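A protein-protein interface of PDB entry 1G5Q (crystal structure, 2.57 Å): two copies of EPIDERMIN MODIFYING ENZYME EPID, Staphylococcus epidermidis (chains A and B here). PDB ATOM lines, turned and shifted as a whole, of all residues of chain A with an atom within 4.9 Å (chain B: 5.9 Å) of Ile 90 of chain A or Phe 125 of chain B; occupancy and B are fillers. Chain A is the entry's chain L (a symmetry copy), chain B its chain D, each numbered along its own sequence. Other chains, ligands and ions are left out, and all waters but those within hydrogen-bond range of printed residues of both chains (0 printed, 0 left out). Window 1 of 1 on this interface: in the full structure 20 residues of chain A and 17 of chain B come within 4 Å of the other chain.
Ile 90 of chain A touches just one residue of chain B: Phe 125 (3.5 Å).
Of the printed residues of chain A, Phe 125 of chain B touches Ile 90 (3.5 Å), Ala 91 (3.1 Å), Gly 93 (3.8 Å), Leu 132 (3.8 Å), Leu 133 (3.6 Å), Asn 136 (3.9 Å) and Val 138 (3.9 Å).
Of the printed residues of chain A, Asn 129 of chain B touches Asn 92 (3.0 Å).
Printed residues of chain A within 4 Å of Asn 88 of chain B: Asn 92 (3.4 Å) and Gly 93 (2.6 Å).
Ile 87 of chain A touches none of the printed residues of chain B.
Ile 130 of chain B touches none of the printed residues of chain A.
The nearest residue of chain B that does not touch Ile 90 of chain A is Asn 123 of chain B (5.5 Å).
The nearest residue of chain A that does not touch Phe 125 of chain B is Asn 92 of chain A (4.2 Å).
The side-chain amide oxygen (OD1) of Asn 123 of chain B sits at hydrogen-bond distance from the backbone NH (N) of Phe 125 of chain B (2.9 Å).
The side-chain amide oxygen (OD1) of Asn 123 of chain B sits at hydrogen-bond distance from the backbone NH (N) of Leu 126 of chain B (3.0 Å).
OD1 of Asn 129 of chain B sits close to O of Phe 125 of chain B (3.3 Å).
O of Asn 88 of chain A lies close to OD1 of Asn 92 of chain A, at 2.9 Å.
O of Leu 132 of chain A is in hydrogen-bond range of ND2 of Asn 136 of chain A (2.7 Å).
The backbone carbonyl oxygen (O) of Leu 133 of chain A is in hydrogen-bond range of the backbone NH (N) of Val 138 of chain A (3.0 Å).
OD1 of Asn 88 of chain B lies close to O of Gly 93 of chain A, at 2.6 Å.
OD1 of Asn 129 of chain B lies close to O of Asn 92 of chain A.
Of the 19 printed residues of chain A, 9 touch a printed residue of chain B.
Hydrophobic or aromatic side chains of chain A within 4 Å of the printed part of chain B: Tyr 107, Leu 132, Leu 133 and Val 138.
Printed residues of chain B that touch a printed residue of chain A: Asn 88, Asn 123, Pro 124, Phe 125, Lys 128 and Asn 129.
Hydrophobic or aromatic side chains of chain B that line the printed part of chain A: Pro 124 and Phe 125.
Among the printed residues, no Asp or Glu carboxylate lies within 4 Å of a Lys or Arg side-chain nitrogen of the other chain.
Among the printed residues, merely in contact across the chains: Ile 90 of chain A with Phe 125 of chain B (3.5 Å), Ala 91 of chain A with Phe 125 of chain B (3.1 Å), Asn 92 of chain A with Asn 88 of chain B (3.4 Å), Gly 93 of chain A with Phe 125 of chain B (3.8 Å), Tyr 107 of chain A with Asn 123 of chain B (3.8 Å), Tyr 107 of chain A with Pro 124 of chain B (3.5 Å), Leu 132 of chain A with Phe 125 of chain B (3.8 Å), Leu 132 of chain A with Lys 128 of chain B (3.3 Å), Leu 133 of chain A with Phe 125 of chain B (3.6 Å), Asn 136 of chain A with Pro 124 of chain B (3.6 Å), Asn 136 of chain A with Phe 125 of chain B (3.9 Å), Asn 136 of chain A with Lys 128 of chain B (3.9 Å) and Val 138 of chain A with Phe 125 of chain B (3.9 Å).
Position printed for both chains: 88.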
ATOM      1  N   VAL A  79      -2.687   2.481  -7.844  1.00  0.00           N
ATOM      2  CA  VAL A  79      -1.842   1.533  -7.141  1.00  0.00           C
ATOM      3  C   VAL A  79      -1.007   1.012  -8.308  1.00  0.00           C
ATOM      4  O   VAL A  79      -1.478   0.229  -9.126  1.00  0.00           O
ATOM      5  CB  VAL A  79      -2.662   0.398  -6.485  1.00  0.00           C
ATOM      6  CG1 VAL A  79      -1.762  -0.439  -5.607  1.00  0.00           C
ATOM      7  CG2 VAL A  79      -3.792   0.986  -5.653  1.00  0.00           C
ATOM      8  N   THR A  86      -0.971  -6.248  -1.686  1.00  0.00           N
ATOM      9  CA  THR A  86      -1.768  -5.038  -1.507  1.00  0.00           C
ATOM     10  C   THR A  86      -3.155  -5.173  -2.127  1.00  0.00           C
ATOM     11  O   THR A  86      -4.141  -4.688  -1.565  1.00  0.00           O
ATOM     12  CB  THR A  86      -1.039  -3.782  -2.081  1.00  0.00           C
ATOM     13  OG1 THR A  86       0.052  -3.433  -1.219  1.00  0.00           O
ATOM     14  CG2 THR A  86      -1.988  -2.585  -2.178  1.00  0.00           C
ATOM     15  N   ILE A  87      -3.236  -5.834  -3.278  1.00  0.00           N
ATOM     16  CA  ILE A  87      -4.527  -6.032  -3.927  1.00  0.00           C
ATOM     17  C   ILE A  87      -5.439  -6.816  -2.977  1.00  0.00           C
ATOM     18  O   ILE A  87      -6.600  -6.457  -2.754  1.00  0.00           O
ATOM     19  CB  ILE A  87      -4.369  -6.816  -5.257  1.00  0.00           C
ATOM     20  CG1 ILE A  87      -3.694  -5.927  -6.308  1.00  0.00           C
ATOM     21  CG2 ILE A  87      -5.727  -7.298  -5.750  1.00  0.00           C
ATOM     22  CD1 ILE A  87      -3.322  -6.647  -7.586  1.00  0.00           C
ATOM     23  N   ASN A  88      -4.900  -7.882  -2.403  1.00  0.00           N
ATOM     24  CA  ASN A  88      -5.671  -8.714  -1.488  1.00  0.00           C
ATOM     25  C   ASN A  88      -6.021  -8.017  -0.181  1.00  0.00           C
ATOM     26  O   ASN A  88      -7.078  -8.283   0.401  1.00  0.00           O
ATOM     27  CB  ASN A  88      -4.916 -10.017  -1.229  1.00  0.00           C
ATOM     28  CG  ASN A  88      -4.860 -10.893  -2.465  1.00  0.00           C
ATOM     29  OD1 ASN A  88      -3.888 -11.608  -2.696  1.00  0.00           O
ATOM     30  ND2 ASN A  88      -5.919 -10.840  -3.268  1.00  0.00           N
ATOM     31  N   LYS A  89      -5.145  -7.129   0.285  1.00  0.00           N
ATOM     32  CA  LYS A  89      -5.421  -6.392   1.514  1.00  0.00           C
ATOM     33  C   LYS A  89      -6.560  -5.416   1.246  1.00  0.00           C
ATOM     34  O   LYS A  89      -7.487  -5.294   2.050  1.00  0.00           O
ATOM     35  CB  LYS A  89      -4.178  -5.629   1.995  1.00  0.00           C
ATOM     36  CG  LYS A  89      -3.141  -6.506   2.691  1.00  0.00           C
ATOM     37  CD  LYS A  89      -2.098  -5.682   3.436  1.00  0.00           C
ATOM     38  CE  LYS A  89      -1.233  -6.570   4.324  1.00  0.00           C
ATOM     39  NZ  LYS A  89      -0.202  -5.822   5.111  1.00  0.00           N
ATOM     40  N   ILE A  90      -6.500  -4.735   0.105  1.00  0.00           N
ATOM     41  CA  ILE A  90      -7.536  -3.774  -0.249  1.00  0.00           C
ATOM     42  C   ILE A  90      -8.878  -4.483  -0.363  1.00  0.00           C
ATOM     43  O   ILE A  90      -9.889  -4.010   0.160  1.00  0.00           O
ATOM     44  CB  ILE A  90      -7.211  -3.066  -1.587  1.00  0.00           C
ATOM     45  CG1 ILE A  90      -5.903  -2.286  -1.448  1.00  0.00           C
ATOM     46  CG2 ILE A  90      -8.345  -2.121  -1.976  1.00  0.00           C
ATOM     47  CD1 ILE A  90      -5.422  -1.669  -2.732  1.00  0.00           C
ATOM     48  N   ALA A  91      -8.883  -5.627  -1.036  1.00  0.00           N
ATOM     49  CA  ALA A  91     -10.108  -6.394  -1.210  1.00  0.00           C
ATOM     50  C   ALA A  91     -10.733  -6.804   0.125  1.00  0.00           C
ATOM     51  O   ALA A  91     -11.961  -6.883   0.244  1.00  0.00           O
ATOM     52  CB  ALA A  91      -9.832  -7.625  -2.059  1.00  0.00           C
ATOM     53  N   ASN A  92      -9.898  -7.072   1.130  1.00  0.00           N
ATOM     54  CA  ASN A  92     -10.423  -7.470   2.436  1.00  0.00           C
ATOM     55  C   ASN A  92     -10.569  -6.315   3.419  1.00  0.00           C
ATOM     56  O   ASN A  92     -10.915  -6.521   4.585  1.00  0.00           O
ATOM     57  CB  ASN A  92      -9.556  -8.566   3.068  1.00  0.00           C
ATOM     58  CG  ASN A  92      -9.691  -9.900   2.357  1.00  0.00           C
ATOM     59  OD1 ASN A  92      -8.834 -10.274   1.553  1.00  0.00           O
ATOM     60  ND2 ASN A  92     -10.778 -10.621   2.641  1.00  0.00           N
ATOM     61  N   GLY A  93     -10.310  -5.102   2.944  1.00  0.00           N
ATOM     62  CA  GLY A  93     -10.440  -3.933   3.797  1.00  0.00           C
ATOM     63  C   GLY A  93      -9.328  -3.813   4.818  1.00  0.00           C
ATOM     64  O   GLY A  93      -9.431  -3.060   5.785  1.00  0.00           O
ATOM     65  N   ILE A  94      -8.254  -4.559   4.617  1.00  0.00           N
ATOM     66  CA  ILE A  94      -7.148  -4.497   5.550  1.00  0.00           C
ATOM     67  C   ILE A  94      -6.276  -3.290   5.257  1.00  0.00           C
ATOM     68  O   ILE A  94      -5.862  -3.066   4.120  1.00  0.00           O
ATOM     69  CB  ILE A  94      -6.340  -5.793   5.494  1.00  0.00           C
ATOM     70  CG1 ILE A  94      -7.202  -6.906   6.086  1.00  0.00           C
ATOM     71  CG2 ILE A  94      -5.030  -5.653   6.261  1.00  0.00           C
ATOM     72  CD1 ILE A  94      -6.663  -8.250   5.865  1.00  0.00           C
ATOM     73  N   THR A 100      -2.321   1.265   2.348  1.00  0.00           N
ATOM     74  CA  THR A 100      -3.589   0.547   2.332  1.00  0.00           C
ATOM     75  C   THR A 100      -4.698   1.318   3.030  1.00  0.00           C
ATOM     76  O   THR A 100      -5.869   1.163   2.689  1.00  0.00           O
ATOM     77  CB  THR A 100      -3.452  -0.857   2.951  1.00  0.00           C
ATOM     78  OG1 THR A 100      -2.848  -0.764   4.243  1.00  0.00           O
ATOM     79  CG2 THR A 100      -2.592  -1.735   2.061  1.00  0.00           C
ATOM     80  N   CYS A 103      -5.970   3.614   0.480  1.00  0.00           N
ATOM     81  CA  CYS A 103      -6.767   2.890  -0.496  1.00  0.00           C
ATOM     82  C   CYS A 103      -8.149   2.525   0.031  1.00  0.00           C
ATOM     83  O   CYS A 103      -9.103   2.483  -0.735  1.00  0.00           O
ATOM     84  CB  CYS A 103      -6.029   1.638  -0.970  1.00  0.00           C
ATOM     85  SG  CYS A 103      -4.553   2.027  -1.950  1.00  0.00           S
ATOM     86  N   TYR A 107     -11.429   4.301  -1.935  1.00  0.00           N
ATOM     87  CA  TYR A 107     -11.825   3.242  -2.861  1.00  0.00           C
ATOM     88  C   TYR A 107     -12.565   3.771  -4.093  1.00  0.00           C
ATOM     89  O   TYR A 107     -12.517   3.161  -5.167  1.00  0.00           O
ATOM     90  CB  TYR A 107     -12.707   2.206  -2.153  1.00  0.00           C
ATOM     91  CG  TYR A 107     -14.036   2.741  -1.664  1.00  0.00           C
ATOM     92  CD1 TYR A 107     -14.103   3.564  -0.539  1.00  0.00           C
ATOM     93  CD2 TYR A 107     -15.230   2.430  -2.329  1.00  0.00           C
ATOM     94  CE1 TYR A 107     -15.320   4.067  -0.083  1.00  0.00           C
ATOM     95  CE2 TYR A 107     -16.458   2.932  -1.879  1.00  0.00           C
ATOM     96  CZ  TYR A 107     -16.492   3.749  -0.755  1.00  0.00           C
ATOM     97  OH  TYR A 107     -17.683   4.257  -0.281  1.00  0.00           O
ATOM     98  N   LEU A 110     -10.006   4.844  -6.777  1.00  0.00           N
ATOM     99  CA  LEU A 110      -8.952   3.858  -6.931  1.00  0.00           C
ATOM    100  C   LEU A 110      -8.821   3.177  -8.293  1.00  0.00           C
ATOM    101  O   LEU A 110      -9.804   2.705  -8.862  1.00  0.00           O
ATOM    102  CB  LEU A 110      -9.132   2.806  -5.833  1.00  0.00           C
ATOM    103  CG  LEU A 110      -7.921   2.105  -5.225  1.00  0.00           C
ATOM    104  CD1 LEU A 110      -6.888   3.134  -4.787  1.00  0.00           C
ATOM    105  CD2 LEU A 110      -8.389   1.268  -4.039  1.00  0.00           C
ATOM    106  N   ILE A 112      -6.306   0.252  -9.954  1.00  0.00           N
ATOM    107  CA  ILE A 112      -5.289  -0.746  -9.657  1.00  0.00           C
ATOM    108  C   ILE A 112      -4.636  -1.379 -10.880  1.00  0.00           C
ATOM    109  O   ILE A 112      -5.319  -1.902 -11.750  1.00  0.00           O
ATOM    110  CB  ILE A 112      -5.900  -1.860  -8.778  1.00  0.00           C
ATOM    111  CG1 ILE A 112      -6.365  -1.257  -7.449  1.00  0.00           C
ATOM    112  CG2 ILE A 112      -4.891  -2.972  -8.542  1.00  0.00           C
ATOM    113  CD1 ILE A 112      -7.048  -2.243  -6.515  1.00  0.00           C
ATOM    114  N   LEU A 132     -14.105  -9.496  -6.523  1.00  0.00           N
ATOM    115  CA  LEU A 132     -14.765  -8.745  -5.466  1.00  0.00           C
ATOM    116  C   LEU A 132     -14.497  -7.251  -5.626  1.00  0.00           C
ATOM    117  O   LEU A 132     -15.392  -6.423  -5.428  1.00  0.00           O
ATOM    118  CB  LEU A 132     -14.271  -9.220  -4.101  1.00  0.00           C
ATOM    119  CG  LEU A 132     -14.912  -8.531  -2.897  1.00  0.00           C
ATOM    120  CD1 LEU A 132     -16.409  -8.816  -2.860  1.00  0.00           C
ATOM    121  CD2 LEU A 132     -14.239  -9.024  -1.631  1.00  0.00           C
ATOM    122  N   LEU A 133     -13.264  -6.908  -5.987  1.00  0.00           N
ATOM    123  CA  LEU A 133     -12.904  -5.509  -6.181  1.00  0.00           C
ATOM    124  C   LEU A 133     -13.690  -4.930  -7.352  1.00  0.00           C
ATOM    125  O   LEU A 133     -14.288  -3.864  -7.240  1.00  0.00           O
ATOM    126  CB  LEU A 133     -11.398  -5.377  -6.438  1.00  0.00           C
ATOM    127  CG  LEU A 133     -10.464  -5.527  -5.230  1.00  0.00           C
ATOM    128  CD1 LEU A 133      -9.050  -5.784  -5.709  1.00  0.00           C
ATOM    129  CD2 LEU A 133     -10.532  -4.281  -4.362  1.00  0.00           C
ATOM    130  N   ASN A 136     -17.355  -4.249  -6.953  1.00  0.00           N
ATOM    131  CA  ASN A 136     -17.655  -3.194  -5.996  1.00  0.00           C
ATOM    132  C   ASN A 136     -17.119  -1.858  -6.458  1.00  0.00           C
ATOM    133  O   ASN A 136     -16.777  -0.990  -5.651  1.00  0.00           O
ATOM    134  CB  ASN A 136     -17.102  -3.560  -4.629  1.00  0.00           C
ATOM    135  CG  ASN A 136     -17.972  -4.567  -3.918  1.00  0.00           C
ATOM    136  OD1 ASN A 136     -19.029  -4.222  -3.391  1.00  0.00           O
ATOM    137  ND2 ASN A 136     -17.548  -5.824  -3.918  1.00  0.00           N
ATOM    138  N   VAL A 138     -14.260  -0.920  -8.002  1.00  0.00           N
ATOM    139  CA  VAL A 138     -12.875  -0.524  -7.863  1.00  0.00           C
ATOM    140  C   VAL A 138     -12.319  -0.923  -9.212  1.00  0.00           C
ATOM    141  O   VAL A 138     -12.461  -2.071  -9.630  1.00  0.00           O
ATOM    142  CB  VAL A 138     -12.155  -1.285  -6.732  1.00  0.00           C
ATOM    143  CG1 VAL A 138     -10.666  -0.991  -6.769  1.00  0.00           C
ATOM    144  CG2 VAL A 138     -12.731  -0.866  -5.391  1.00  0.00           C
ATOM    145  N   ASN B  88     -11.622  -5.361  10.152  1.00  0.00           N
ATOM    146  CA  ASN B  88     -11.432  -6.206   8.979  1.00  0.00           C
ATOM    147  C   ASN B  88     -10.472  -7.368   9.209  1.00  0.00           C
ATOM    148  O   ASN B  88     -10.623  -8.440   8.607  1.00  0.00           O
ATOM    149  CB  ASN B  88     -10.981  -5.346   7.802  1.00  0.00           C
ATOM    150  CG  ASN B  88     -12.071  -4.393   7.343  1.00  0.00           C
ATOM    151  OD1 ASN B  88     -11.797  -3.260   6.934  1.00  0.00           O
ATOM    152  ND2 ASN B  88     -13.324  -4.850   7.410  1.00  0.00           N
ATOM    153  N   ASN B 123     -16.996   2.089   3.104  1.00  0.00           N
ATOM    154  CA  ASN B 123     -16.225   1.122   2.327  1.00  0.00           C
ATOM    155  C   ASN B 123     -16.975  -0.210   2.209  1.00  0.00           C
ATOM    156  O   ASN B 123     -17.371  -0.801   3.208  1.00  0.00           O
ATOM    157  CB  ASN B 123     -14.850   0.923   2.973  1.00  0.00           C
ATOM    158  CG  ASN B 123     -13.965  -0.006   2.184  1.00  0.00           C
ATOM    159  OD1 ASN B 123     -14.170  -1.221   2.166  1.00  0.00           O
ATOM    160  ND2 ASN B 123     -12.972   0.561   1.517  1.00  0.00           N
ATOM    161  N   PRO B 124     -17.161  -0.705   0.971  1.00  0.00           N
ATOM    162  CA  PRO B 124     -17.868  -1.959   0.693  1.00  0.00           C
ATOM    163  C   PRO B 124     -17.290  -3.160   1.433  1.00  0.00           C
ATOM    164  O   PRO B 124     -18.022  -3.953   2.035  1.00  0.00           O
ATOM    165  CB  PRO B 124     -17.725  -2.121  -0.826  1.00  0.00           C
ATOM    166  CG  PRO B 124     -17.418  -0.752  -1.317  1.00  0.00           C
ATOM    167  CD  PRO B 124     -16.520  -0.198  -0.254  1.00  0.00           C
ATOM    168  N   PHE B 125     -15.972  -3.292   1.363  1.00  0.00           N
ATOM    169  CA  PHE B 125     -15.264  -4.400   1.988  1.00  0.00           C
ATOM    170  C   PHE B 125     -15.401  -4.374   3.505  1.00  0.00           C
ATOM    171  O   PHE B 125     -15.569  -5.415   4.143  1.00  0.00           O
ATOM    172  CB  PHE B 125     -13.812  -4.353   1.536  1.00  0.00           C
ATOM    173  CG  PHE B 125     -13.677  -4.086   0.070  1.00  0.00           C
ATOM    174  CD1 PHE B 125     -13.130  -2.894  -0.387  1.00  0.00           C
ATOM    175  CD2 PHE B 125     -14.199  -4.988  -0.859  1.00  0.00           C
ATOM    176  CE1 PHE B 125     -13.108  -2.599  -1.749  1.00  0.00           C
ATOM    177  CE2 PHE B 125     -14.181  -4.701  -2.222  1.00  0.00           C
ATOM    178  CZ  PHE B 125     -13.637  -3.504  -2.666  1.00  0.00           C
ATOM    179  N   LEU B 126     -15.348  -3.181   4.079  1.00  0.00           N
ATOM    180  CA  LEU B 126     -15.514  -3.050   5.511  1.00  0.00           C
ATOM    181  C   LEU B 126     -16.913  -3.563   5.858  1.00  0.00           C
ATOM    182  O   LEU B 126     -17.075  -4.408   6.745  1.00  0.00           O
ATOM    183  CB  LEU B 126     -15.385  -1.586   5.938  1.00  0.00           C
ATOM    184  CG  LEU B 126     -15.865  -1.290   7.367  1.00  0.00           C
ATOM    185  CD1 LEU B 126     -15.035  -2.089   8.364  1.00  0.00           C
ATOM    186  CD2 LEU B 126     -15.753   0.195   7.659  1.00  0.00           C
ATOM    187  N   GLN B 127     -17.919  -3.065   5.144  1.00  0.00           N
ATOM    188  CA  GLN B 127     -19.295  -3.463   5.403  1.00  0.00           C
ATOM    189  C   GLN B 127     -19.575  -4.956   5.246  1.00  0.00           C
ATOM    190  O   GLN B 127     -20.369  -5.515   6.007  1.00  0.00           O
ATOM    191  CB  GLN B 127     -20.246  -2.647   4.536  1.00  0.00           C
ATOM    192  CG  GLN B 127     -20.366  -1.201   4.990  1.00  0.00           C
ATOM    193  CD  GLN B 127     -20.722  -1.088   6.467  1.00  0.00           C
ATOM    194  OE1 GLN B 127     -21.569  -1.830   6.972  1.00  0.00           O
ATOM    195  NE2 GLN B 127     -20.081  -0.149   7.167  1.00  0.00           N
ATOM    196  N   LYS B 128     -18.938  -5.608   4.279  1.00  0.00           N
ATOM    197  CA  LYS B 128     -19.160  -7.040   4.115  1.00  0.00           C
ATOM    198  C   LYS B 128     -18.627  -7.782   5.332  1.00  0.00           C
ATOM    199  O   LYS B 128     -19.228  -8.763   5.784  1.00  0.00           O
ATOM    200  CB  LYS B 128     -18.489  -7.570   2.841  1.00  0.00           C
ATOM    201  CG  LYS B 128     -19.195  -7.116   1.572  1.00  0.00           C
ATOM    202  CD  LYS B 128     -18.885  -7.997   0.363  1.00  0.00           C
ATOM    203  CE  LYS B 128     -19.817  -7.640  -0.803  1.00  0.00           C
ATOM    204  NZ  LYS B 128     -19.618  -8.493  -2.017  1.00  0.00           N
ATOM    205  N   ASN B 129     -17.507  -7.294   5.870  1.00  0.00           N
ATOM    206  CA  ASN B 129     -16.882  -7.888   7.046  1.00  0.00           C
ATOM    207  C   ASN B 129     -17.728  -7.664   8.305  1.00  0.00           C
ATOM    208  O   ASN B 129     -17.793  -8.528   9.186  1.00  0.00           O
ATOM    209  CB  ASN B 129     -15.488  -7.297   7.237  1.00  0.00           C
ATOM    210  CG  ASN B 129     -14.501  -7.786   6.201  1.00  0.00           C
ATOM    211  OD1 ASN B 129     -13.456  -7.168   5.986  1.00  0.00           O
ATOM    212  ND2 ASN B 129     -14.816  -8.903   5.560  1.00  0.00           N
ATOM    213  N   ILE B 130     -18.371  -6.506   8.388  1.00  0.00           N
ATOM    214  CA  ILE B 130     -19.219  -6.212   9.527  1.00  0.00           C
ATOM    215  C   ILE B 130     -20.439  -7.135   9.546  1.00  0.00           C
ATOM    216  O   ILE B 130     -20.921  -7.518  10.615  1.00  0.00           O
ATOM    217  CB  ILE B 130     -19.655  -4.733   9.516  1.00  0.00           C
ATOM    218  CG1 ILE B 130     -18.505  -3.886  10.070  1.00  0.00           C
ATOM    219  CG2 ILE B 130     -20.935  -4.538  10.325  1.00  0.00           C
ATOM    220  CD1 ILE B 130     -18.797  -2.433  10.172  1.00  0.00           C
